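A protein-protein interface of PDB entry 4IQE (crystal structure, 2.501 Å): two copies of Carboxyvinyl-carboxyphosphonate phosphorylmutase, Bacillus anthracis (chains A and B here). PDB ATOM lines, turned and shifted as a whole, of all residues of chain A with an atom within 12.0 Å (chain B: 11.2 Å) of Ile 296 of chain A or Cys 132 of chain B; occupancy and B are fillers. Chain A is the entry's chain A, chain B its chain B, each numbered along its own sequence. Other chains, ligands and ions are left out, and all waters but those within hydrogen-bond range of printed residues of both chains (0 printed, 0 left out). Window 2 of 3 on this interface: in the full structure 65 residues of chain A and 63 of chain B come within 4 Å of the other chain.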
ATOM      1  N   VAL A   7      -1.081 -13.578  11.747  1.00  0.00           N
ATOM      2  CA  VAL A   7      -1.814 -14.251  10.681  1.00  0.00           C
ATOM      3  C   VAL A   7      -2.078 -13.326   9.496  1.00  0.00           C
ATOM      4  O   VAL A   7      -2.831 -13.670   8.584  1.00  0.00           O
ATOM      5  CB  VAL A   7      -3.153 -14.824  11.184  1.00  0.00           C
ATOM      6  CG1 VAL A   7      -2.915 -16.071  12.017  1.00  0.00           C
ATOM      7  CG2 VAL A   7      -3.917 -13.773  11.975  1.00  0.00           C
ATOM      8  N   VAL A   8      -1.456 -12.152   9.516  1.00  0.00           N
ATOM      9  CA  VAL A   8      -1.575 -11.204   8.413  1.00  0.00           C
ATOM     10  C   VAL A   8      -0.349 -11.276   7.504  1.00  0.00           C
ATOM     11  O   VAL A   8       0.700 -10.705   7.812  1.00  0.00           O
ATOM     12  CB  VAL A   8      -1.755  -9.762   8.923  1.00  0.00           C
ATOM     13  CG1 VAL A   8      -1.879  -8.798   7.753  1.00  0.00           C
ATOM     14  CG2 VAL A   8      -2.974  -9.671   9.825  1.00  0.00           C
ATOM     15  N   ASN A   9      -0.495 -11.985   6.387  1.00  0.00           N
ATOM     16  CA  ASN A   9       0.600 -12.205   5.440  1.00  0.00           C
ATOM     17  C   ASN A   9       1.869 -12.740   6.093  1.00  0.00           C
ATOM     18  O   ASN A   9       1.807 -13.483   7.071  1.00  0.00           O
ATOM     19  CB  ASN A   9       0.905 -10.934   4.644  1.00  0.00           C
ATOM     20  CG  ASN A   9      -0.092 -10.693   3.529  1.00  0.00           C
ATOM     21  OD1 ASN A   9      -0.749 -11.622   3.060  1.00  0.00           O
ATOM     22  ND2 ASN A   9      -0.204  -9.444   3.095  1.00  0.00           N
ATOM     23  N   TYR A 286      -2.161  -4.463  15.634  1.00  0.00           N
ATOM     24  CA  TYR A 286      -3.606  -4.262  15.563  1.00  0.00           C
ATOM     25  C   TYR A 286      -3.997  -3.654  14.221  1.00  0.00           C
ATOM     26  O   TYR A 286      -5.033  -3.996  13.656  1.00  0.00           O
ATOM     27  CB  TYR A 286      -4.077  -3.356  16.707  1.00  0.00           C
ATOM     28  CG  TYR A 286      -5.576  -3.113  16.754  1.00  0.00           C
ATOM     29  CD1 TYR A 286      -6.395  -3.865  17.585  1.00  0.00           C
ATOM     30  CD2 TYR A 286      -6.169  -2.123  15.974  1.00  0.00           C
ATOM     31  CE1 TYR A 286      -7.761  -3.643  17.634  1.00  0.00           C
ATOM     32  CE2 TYR A 286      -7.531  -1.897  16.017  1.00  0.00           C
ATOM     33  CZ  TYR A 286      -8.323  -2.659  16.848  1.00  0.00           C
ATOM     34  OH  TYR A 286      -9.682  -2.439  16.895  1.00  0.00           O
ATOM     35  N   HIS A 287      -3.160  -2.748  13.721  1.00  0.00           N
ATOM     36  CA  HIS A 287      -3.428  -2.053  12.467  1.00  0.00           C
ATOM     37  C   HIS A 287      -3.506  -3.019  11.288  1.00  0.00           C
ATOM     38  O   HIS A 287      -4.288  -2.815  10.359  1.00  0.00           O
ATOM     39  CB  HIS A 287      -2.355  -0.991  12.209  1.00  0.00           C
ATOM     40  CG  HIS A 287      -2.622  -0.138  11.006  1.00  0.00           C
ATOM     41  ND1 HIS A 287      -1.900  -0.249   9.839  1.00  0.00           N
ATOM     42  CD2 HIS A 287      -3.534   0.842  10.795  1.00  0.00           C
ATOM     43  CE1 HIS A 287      -2.354   0.626   8.957  1.00  0.00           C
ATOM     44  NE2 HIS A 287      -3.345   1.299   9.512  1.00  0.00           N
ATOM     45  N   ASP A 288      -2.695  -4.072  11.334  1.00  0.00           N
ATOM     46  CA  ASP A 288      -2.664  -5.062  10.263  1.00  0.00           C
ATOM     47  C   ASP A 288      -3.880  -5.985  10.310  1.00  0.00           C
ATOM     48  O   ASP A 288      -4.310  -6.510   9.285  1.00  0.00           O
ATOM     49  CB  ASP A 288      -1.364  -5.868  10.308  1.00  0.00           C
ATOM     50  CG  ASP A 288      -0.139  -5.008  10.059  1.00  0.00           C
ATOM     51  OD1 ASP A 288       0.953  -5.364  10.550  1.00  0.00           O
ATOM     52  OD2 ASP A 288      -0.271  -3.973   9.375  1.00  0.00           O
ATOM     53  N   PHE A 289      -4.430  -6.175  11.505  1.00  0.00           N
ATOM     54  CA  PHE A 289      -5.657  -6.943  11.663  1.00  0.00           C
ATOM     55  C   PHE A 289      -6.848  -6.104  11.229  1.00  0.00           C
ATOM     56  O   PHE A 289      -7.861  -6.635  10.775  1.00  0.00           O
ATOM     57  CB  PHE A 289      -5.839  -7.393  13.115  1.00  0.00           C
ATOM     58  CG  PHE A 289      -5.033  -8.605  13.482  1.00  0.00           C
ATOM     59  CD1 PHE A 289      -5.629  -9.854  13.558  1.00  0.00           C
ATOM     60  CD2 PHE A 289      -3.680  -8.498  13.746  1.00  0.00           C
ATOM     61  CE1 PHE A 289      -4.887 -10.971  13.896  1.00  0.00           C
ATOM     62  CE2 PHE A 289      -2.933  -9.609  14.082  1.00  0.00           C
ATOM     63  CZ  PHE A 289      -3.536 -10.847  14.158  1.00  0.00           C
ATOM     64  N   GLU A 290      -6.717  -4.789  11.368  1.00  0.00           N
ATOM     65  CA  GLU A 290      -7.791  -3.873  11.004  1.00  0.00           C
ATOM     66  C   GLU A 290      -7.875  -3.696   9.492  1.00  0.00           C
ATOM     67  O   GLU A 290      -8.959  -3.758   8.918  1.00  0.00           O
ATOM     68  CB  GLU A 290      -7.605  -2.517  11.688  1.00  0.00           C
ATOM     69  CG  GLU A 290      -8.833  -1.622  11.624  1.00  0.00           C
ATOM     70  CD  GLU A 290      -8.575  -0.236  12.180  1.00  0.00           C
ATOM     71  OE1 GLU A 290      -9.263   0.715  11.753  1.00  0.00           O
ATOM     72  OE2 GLU A 290      -7.685  -0.096  13.046  1.00  0.00           O
ATOM     73  N   GLU A 291      -6.728  -3.482   8.852  1.00  0.00           N
ATOM     74  CA  GLU A 291      -6.681  -3.308   7.402  1.00  0.00           C
ATOM     75  C   GLU A 291      -7.117  -4.579   6.678  1.00  0.00           C
ATOM     76  O   GLU A 291      -7.608  -4.526   5.551  1.00  0.00           O
ATOM     77  CB  GLU A 291      -5.276  -2.900   6.949  1.00  0.00           C
ATOM     78  CG  GLU A 291      -4.201  -3.922   7.270  1.00  0.00           C
ATOM     79  CD  GLU A 291      -3.367  -4.296   6.063  1.00  0.00           C
ATOM     80  OE1 GLU A 291      -3.271  -3.476   5.127  1.00  0.00           O
ATOM     81  OE2 GLU A 291      -2.812  -5.416   6.048  1.00  0.00           O
ATOM     82  N   LEU A 292      -6.929  -5.721   7.334  1.00  0.00           N
ATOM     83  CA  LEU A 292      -7.362  -7.004   6.797  1.00  0.00           C
ATOM     84  C   LEU A 292      -8.881  -7.066   6.767  1.00  0.00           C
ATOM     85  O   LEU A 292      -9.488  -7.245   5.711  1.00  0.00           O
ATOM     86  CB  LEU A 292      -6.820  -8.148   7.654  1.00  0.00           C
ATOM     87  CG  LEU A 292      -7.466  -9.523   7.456  1.00  0.00           C
ATOM     88  CD1 LEU A 292      -7.202 -10.053   6.058  1.00  0.00           C
ATOM     89  CD2 LEU A 292      -6.977 -10.506   8.509  1.00  0.00           C
ATOM     90  N   ASP A 293      -9.481  -6.912   7.942  1.00  0.00           N
ATOM     91  CA  ASP A 293     -10.930  -6.953   8.100  1.00  0.00           C
ATOM     92  C   ASP A 293     -11.635  -5.858   7.302  1.00  0.00           C
ATOM     93  O   ASP A 293     -12.662  -6.106   6.675  1.00  0.00           O
ATOM     94  CB  ASP A 293     -11.293  -6.857   9.585  1.00  0.00           C
ATOM     95  CG  ASP A 293     -12.607  -6.143   9.821  1.00  0.00           C
ATOM     96  OD1 ASP A 293     -13.661  -6.811   9.815  1.00  0.00           O
ATOM     97  OD2 ASP A 293     -12.583  -4.911  10.023  1.00  0.00           O
ATOM     98  N   THR A 294     -11.077  -4.651   7.329  1.00  0.00           N
ATOM     99  CA  THR A 294     -11.644  -3.525   6.590  1.00  0.00           C
ATOM    100  C   THR A 294     -11.459  -3.705   5.084  1.00  0.00           C
ATOM    101  O   THR A 294     -12.330  -3.344   4.292  1.00  0.00           O
ATOM    102  CB  THR A 294     -11.020  -2.185   7.039  1.00  0.00           C
ATOM    103  OG1 THR A 294     -11.277  -1.983   8.435  1.00  0.00           O
ATOM    104  CG2 THR A 294     -11.599  -1.018   6.251  1.00  0.00           C
ATOM    105  N   GLY A 295     -10.320  -4.268   4.697  1.00  0.00           N
ATOM    106  CA  GLY A 295     -10.039  -4.541   3.299  1.00  0.00           C
ATOM    107  C   GLY A 295     -11.037  -5.522   2.720  1.00  0.00           C
ATOM    108  O   GLY A 295     -11.472  -5.381   1.577  1.00  0.00           O
ATOM    109  N   ILE A 296     -11.398  -6.522   3.517  1.00  0.00           N
ATOM    110  CA  ILE A 296     -12.422  -7.485   3.132  1.00  0.00           C
ATOM    111  C   ILE A 296     -13.792  -6.812   3.180  1.00  0.00           C
ATOM    112  O   ILE A 296     -14.662  -7.079   2.348  1.00  0.00           O
ATOM    113  CB  ILE A 296     -12.394  -8.739   4.049  1.00  0.00           C
ATOM    114  CG1 ILE A 296     -11.484  -9.821   3.457  1.00  0.00           C
ATOM    115  CG2 ILE A 296     -13.790  -9.312   4.252  1.00  0.00           C
ATOM    116  CD1 ILE A 296     -10.019  -9.446   3.392  1.00  0.00           C
ATOM    117  N   ALA A 297     -13.960  -5.917   4.148  1.00  0.00           N
ATOM    118  CA  ALA A 297     -15.215  -5.197   4.343  1.00  0.00           C
ATOM    119  C   ALA A 297     -15.608  -4.353   3.134  1.00  0.00           C
ATOM    120  O   ALA A 297     -16.728  -4.456   2.638  1.00  0.00           O
ATOM    121  CB  ALA A 297     -15.132  -4.323   5.583  1.00  0.00           C
ATOM    122  N   LYS A 298     -14.686  -3.519   2.664  1.00  0.00           N
ATOM    123  CA  LYS A 298     -15.012  -2.561   1.611  1.00  0.00           C
ATOM    124  C   LYS A 298     -14.980  -3.192   0.220  1.00  0.00           C
ATOM    125  O   LYS A 298     -15.129  -2.505  -0.790  1.00  0.00           O
ATOM    126  CB  LYS A 298     -14.094  -1.333   1.675  1.00  0.00           C
ATOM    127  CG  LYS A 298     -13.886  -0.759   3.079  1.00  0.00           C
ATOM    128  CD  LYS A 298     -15.172  -0.707   3.914  1.00  0.00           C
ATOM    129  CE  LYS A 298     -16.211   0.263   3.369  1.00  0.00           C
ATOM    130  NZ  LYS A 298     -17.477   0.159   4.153  1.00  0.00           N
ATOM    131  N   THR A 299     -14.798  -4.506   0.176  1.00  0.00           N
ATOM    132  CA  THR A 299     -14.828  -5.241  -1.080  1.00  0.00           C
ATOM    133  C   THR A 299     -15.968  -6.254  -1.090  1.00  0.00           C
ATOM    134  O   THR A 299     -17.131  -5.897  -0.897  1.00  0.00           O
ATOM    135  CB  THR A 299     -13.498  -5.966  -1.347  1.00  0.00           C
ATOM    136  OG1 THR A 299     -13.123  -6.719  -0.188  1.00  0.00           O
ATOM    137  CG2 THR A 299     -12.402  -4.963  -1.669  1.00  0.00           C
ATOM    138  N   LEU B  69      -9.067  -9.514  20.292  1.00  0.00           N
ATOM    139  CA  LEU B  69     -10.176  -9.416  19.354  1.00  0.00           C
ATOM    140  C   LEU B  69     -11.040 -10.673  19.377  1.00  0.00           C
ATOM    141  O   LEU B  69     -11.663 -11.022  18.374  1.00  0.00           O
ATOM    142  CB  LEU B  69      -9.653  -9.158  17.940  1.00  0.00           C
ATOM    143  CG  LEU B  69      -8.886  -7.848  17.746  1.00  0.00           C
ATOM    144  CD1 LEU B  69      -8.257  -7.778  16.364  1.00  0.00           C
ATOM    145  CD2 LEU B  69      -9.797  -6.653  17.984  1.00  0.00           C
ATOM    146  N   GLN B 127     -21.154  -7.424  22.288  1.00  0.00           N
ATOM    147  CA  GLN B 127     -21.702  -8.259  21.229  1.00  0.00           C
ATOM    148  C   GLN B 127     -20.593  -8.710  20.284  1.00  0.00           C
ATOM    149  O   GLN B 127     -19.901  -7.888  19.683  1.00  0.00           O
ATOM    150  CB  GLN B 127     -22.798  -7.506  20.469  1.00  0.00           C
ATOM    151  CG  GLN B 127     -23.047  -7.995  19.053  1.00  0.00           C
ATOM    152  CD  GLN B 127     -22.336  -7.147  18.015  1.00  0.00           C
ATOM    153  OE1 GLN B 127     -22.451  -7.389  16.814  1.00  0.00           O
ATOM    154  NE2 GLN B 127     -21.596  -6.146  18.476  1.00  0.00           N
ATOM    155  N   LEU B 128     -20.423 -10.022  20.169  1.00  0.00           N
ATOM    156  CA  LEU B 128     -19.368 -10.589  19.339  1.00  0.00           C
ATOM    157  C   LEU B 128     -19.932 -11.633  18.384  1.00  0.00           C
ATOM    158  O   LEU B 128     -20.861 -12.361  18.733  1.00  0.00           O
ATOM    159  CB  LEU B 128     -18.278 -11.211  20.215  1.00  0.00           C
ATOM    160  CG  LEU B 128     -17.473 -10.240  21.081  1.00  0.00           C
ATOM    161  CD1 LEU B 128     -16.493 -10.989  21.973  1.00  0.00           C
ATOM    162  CD2 LEU B 128     -16.745  -9.223  20.214  1.00  0.00           C
ATOM    163  N   PRO B 129     -19.367 -11.715  17.169  1.00  0.00           N
ATOM    164  CA  PRO B 129     -18.276 -10.867  16.676  1.00  0.00           C
ATOM    165  C   PRO B 129     -18.787  -9.541  16.122  1.00  0.00           C
ATOM    166  O   PRO B 129     -19.985  -9.392  15.882  1.00  0.00           O
ATOM    167  CB  PRO B 129     -17.671 -11.697  15.532  1.00  0.00           C
ATOM    168  CG  PRO B 129     -18.333 -13.052  15.608  1.00  0.00           C
ATOM    169  CD  PRO B 129     -19.659 -12.812  16.237  1.00  0.00           C
ATOM    170  N   LYS B 130     -17.879  -8.592  15.929  1.00  0.00           N
ATOM    171  CA  LYS B 130     -18.214  -7.326  15.291  1.00  0.00           C
ATOM    172  C   LYS B 130     -18.198  -7.509  13.778  1.00  0.00           C
ATOM    173  O   LYS B 130     -17.363  -8.242  13.248  1.00  0.00           O
ATOM    174  CB  LYS B 130     -17.230  -6.233  15.717  1.00  0.00           C
ATOM    175  CG  LYS B 130     -17.268  -4.977  14.858  1.00  0.00           C
ATOM    176  CD  LYS B 130     -16.814  -3.752  15.634  1.00  0.00           C
ATOM    177  CE  LYS B 130     -16.702  -2.536  14.728  1.00  0.00           C
ATOM    178  NZ  LYS B 130     -15.549  -2.651  13.792  1.00  0.00           N
ATOM    179  N   LYS B 131     -19.128  -6.852  13.088  1.00  0.00           N
ATOM    180  CA  LYS B 131     -19.223  -6.967  11.636  1.00  0.00           C
ATOM    181  C   LYS B 131     -17.954  -6.455  10.960  1.00  0.00           C
ATOM    182  O   LYS B 131     -17.091  -5.854  11.603  1.00  0.00           O
ATOM    183  CB  LYS B 131     -20.442  -6.211  11.101  1.00  0.00           C
ATOM    184  CG  LYS B 131     -20.264  -4.701  11.035  1.00  0.00           C
ATOM    185  CD  LYS B 131     -21.379  -4.049  10.231  1.00  0.00           C
ATOM    186  CE  LYS B 131     -22.744  -4.334  10.837  1.00  0.00           C
ATOM    187  NZ  LYS B 131     -23.829  -3.723  10.016  1.00  0.00           N
ATOM    188  N   CYS B 132     -17.857  -6.690   9.656  1.00  0.00           N
ATOM    189  CA  CYS B 132     -16.663  -6.345   8.890  1.00  0.00           C
ATOM    190  C   CYS B 132     -16.278  -4.868   8.977  1.00  0.00           C
ATOM    191  O   CYS B 132     -15.115  -4.513   8.792  1.00  0.00           O
ATOM    192  CB  CYS B 132     -16.824  -6.773   7.431  1.00  0.00           C
ATOM    193  SG  CYS B 132     -16.006  -8.328   7.020  1.00  0.00           S
ATOM    194  N   GLY B 133     -17.253  -4.014   9.264  1.00  0.00           N
ATOM    195  CA  GLY B 133     -16.993  -2.595   9.428  1.00  0.00           C
ATOM    196  C   GLY B 133     -16.360  -2.284  10.770  1.00  0.00           C
ATOM    197  O   GLY B 133     -16.209  -1.121  11.142  1.00  0.00           O
ATOM    198  N   ASN B 136     -12.190  -0.142  14.882  1.00  0.00           N
ATOM    199  CA  ASN B 136     -12.794   0.223  16.157  1.00  0.00           C
ATOM    200  C   ASN B 136     -14.317   0.195  16.102  1.00  0.00           C
ATOM    201  O   ASN B 136     -14.912   0.276  15.027  1.00  0.00           O
ATOM    202  CB  ASN B 136     -12.308   1.603  16.606  1.00  0.00           C
ATOM    203  CG  ASN B 136     -10.813   1.643  16.842  1.00  0.00           C
ATOM    204  OD1 ASN B 136     -10.207   0.642  17.223  1.00  0.00           O
ATOM    205  ND2 ASN B 136     -10.208   2.803  16.615  1.00  0.00           N
ATOM    206  N   GLY B 137     -14.940   0.081  17.271  1.00  0.00           N
ATOM    207  CA  GLY B 137     -16.386   0.041  17.373  1.00  0.00           C
ATOM    208  C   GLY B 137     -16.840  -0.490  18.719  1.00  0.00           C
ATOM    209  O   GLY B 137     -16.059  -1.101  19.448  1.00  0.00           O
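The backbone carbonyl oxygen of Ile 296 of chain A lies within hydrogen-bond range of the side-chain hydroxyl of Thr 299 of chain A (3.0 Å). The backbone carbonyl oxygen (O) of Asn 136 of chain B is in hydrogen-bond range of the side-chain amino group (NZ) of Lys 130 of chain B (3.2 Å).
Of the 17 printed residues of chain A, 4 touch a printed residue of chain B. Printed residues of chain A that touch a printed residue of chain B: Tyr 286, Asp 293, Ile 296 and Ala 297. Hydrophobic or aromatic side chains of chain A within 4 Å of the printed part of chain B: Tyr 286, Ile 296 and Ala 297. Hydrophobic or aromatic side chains of chain B that line the printed part of chain A: Leu 69. Among the printed residues, no Asp or Glu carboxylate lies within 4 Å of a Lys or Arg side-chain nitrogen of the other chain.
Tyr 286 of chain A touches Leu 69 of chain B. Asp 293 of chain A touches Lys 131 of chain B. CG2 of Ile 296 of chain A touches SG of Cys 132 of chain B (3.7 Å). CB of Ala 297 of chain A touches O of Cys 132 of chain B, at 3.2 Å.
No position is printed for both chains. Of the 6 pairs that touch across the chains among the printed residues, none has its exchanged pair printed and touching as well.
The side-chain amide oxygen of Asn 136 of chain B is in hydrogen-bond range of the side-chain hydroxyl of Tyr 286 of chain A (3.1 Å). The backbone carbonyl oxygen of Cys 132 of chain B lies close to the side-chain carboxylate of Asp 293 of chain A.
Ile 296 of chain A touches just one residue of chain B: Cys 132. Of chain A, only Asp 293 (2.8 Å), Ile 296 (3.7 Å) and Ala 297 (3.2 Å) come within 4 Å of Cys 132 of chain B. No residue of chain B comes within 4 Å of Leu 292 of chain A. No residue of chain B comes within 4 Å of Thr 294 of chain A. No residue of chain B comes within 4 Å of Gly 295 of chain A. Of the printed residues of chain B, Ala 297 of chain A touches Cys 132 (3.2 Å). No residue of chain B comes within 4 Å of Thr 299 of chain A. No residue of chain A comes within 4 Å of Lys 130 of chain B. Of the printed residues of chain A, Asn 136 of chain B touches Tyr 286 (3.1 Å). Printed residues of chain A within 4 Å of Lys 131 of chain B: Asp 293 (3.98 Å). Of the printed residues of chain B, Tyr 286 of chain A touches Leu 69 and Asn 136. His 287 of chain A touches none of the printed residues of chain B. The nearest residue of chain A that does not touch Cys 132 of chain B is Thr 294 of chain A (4.2 Å).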
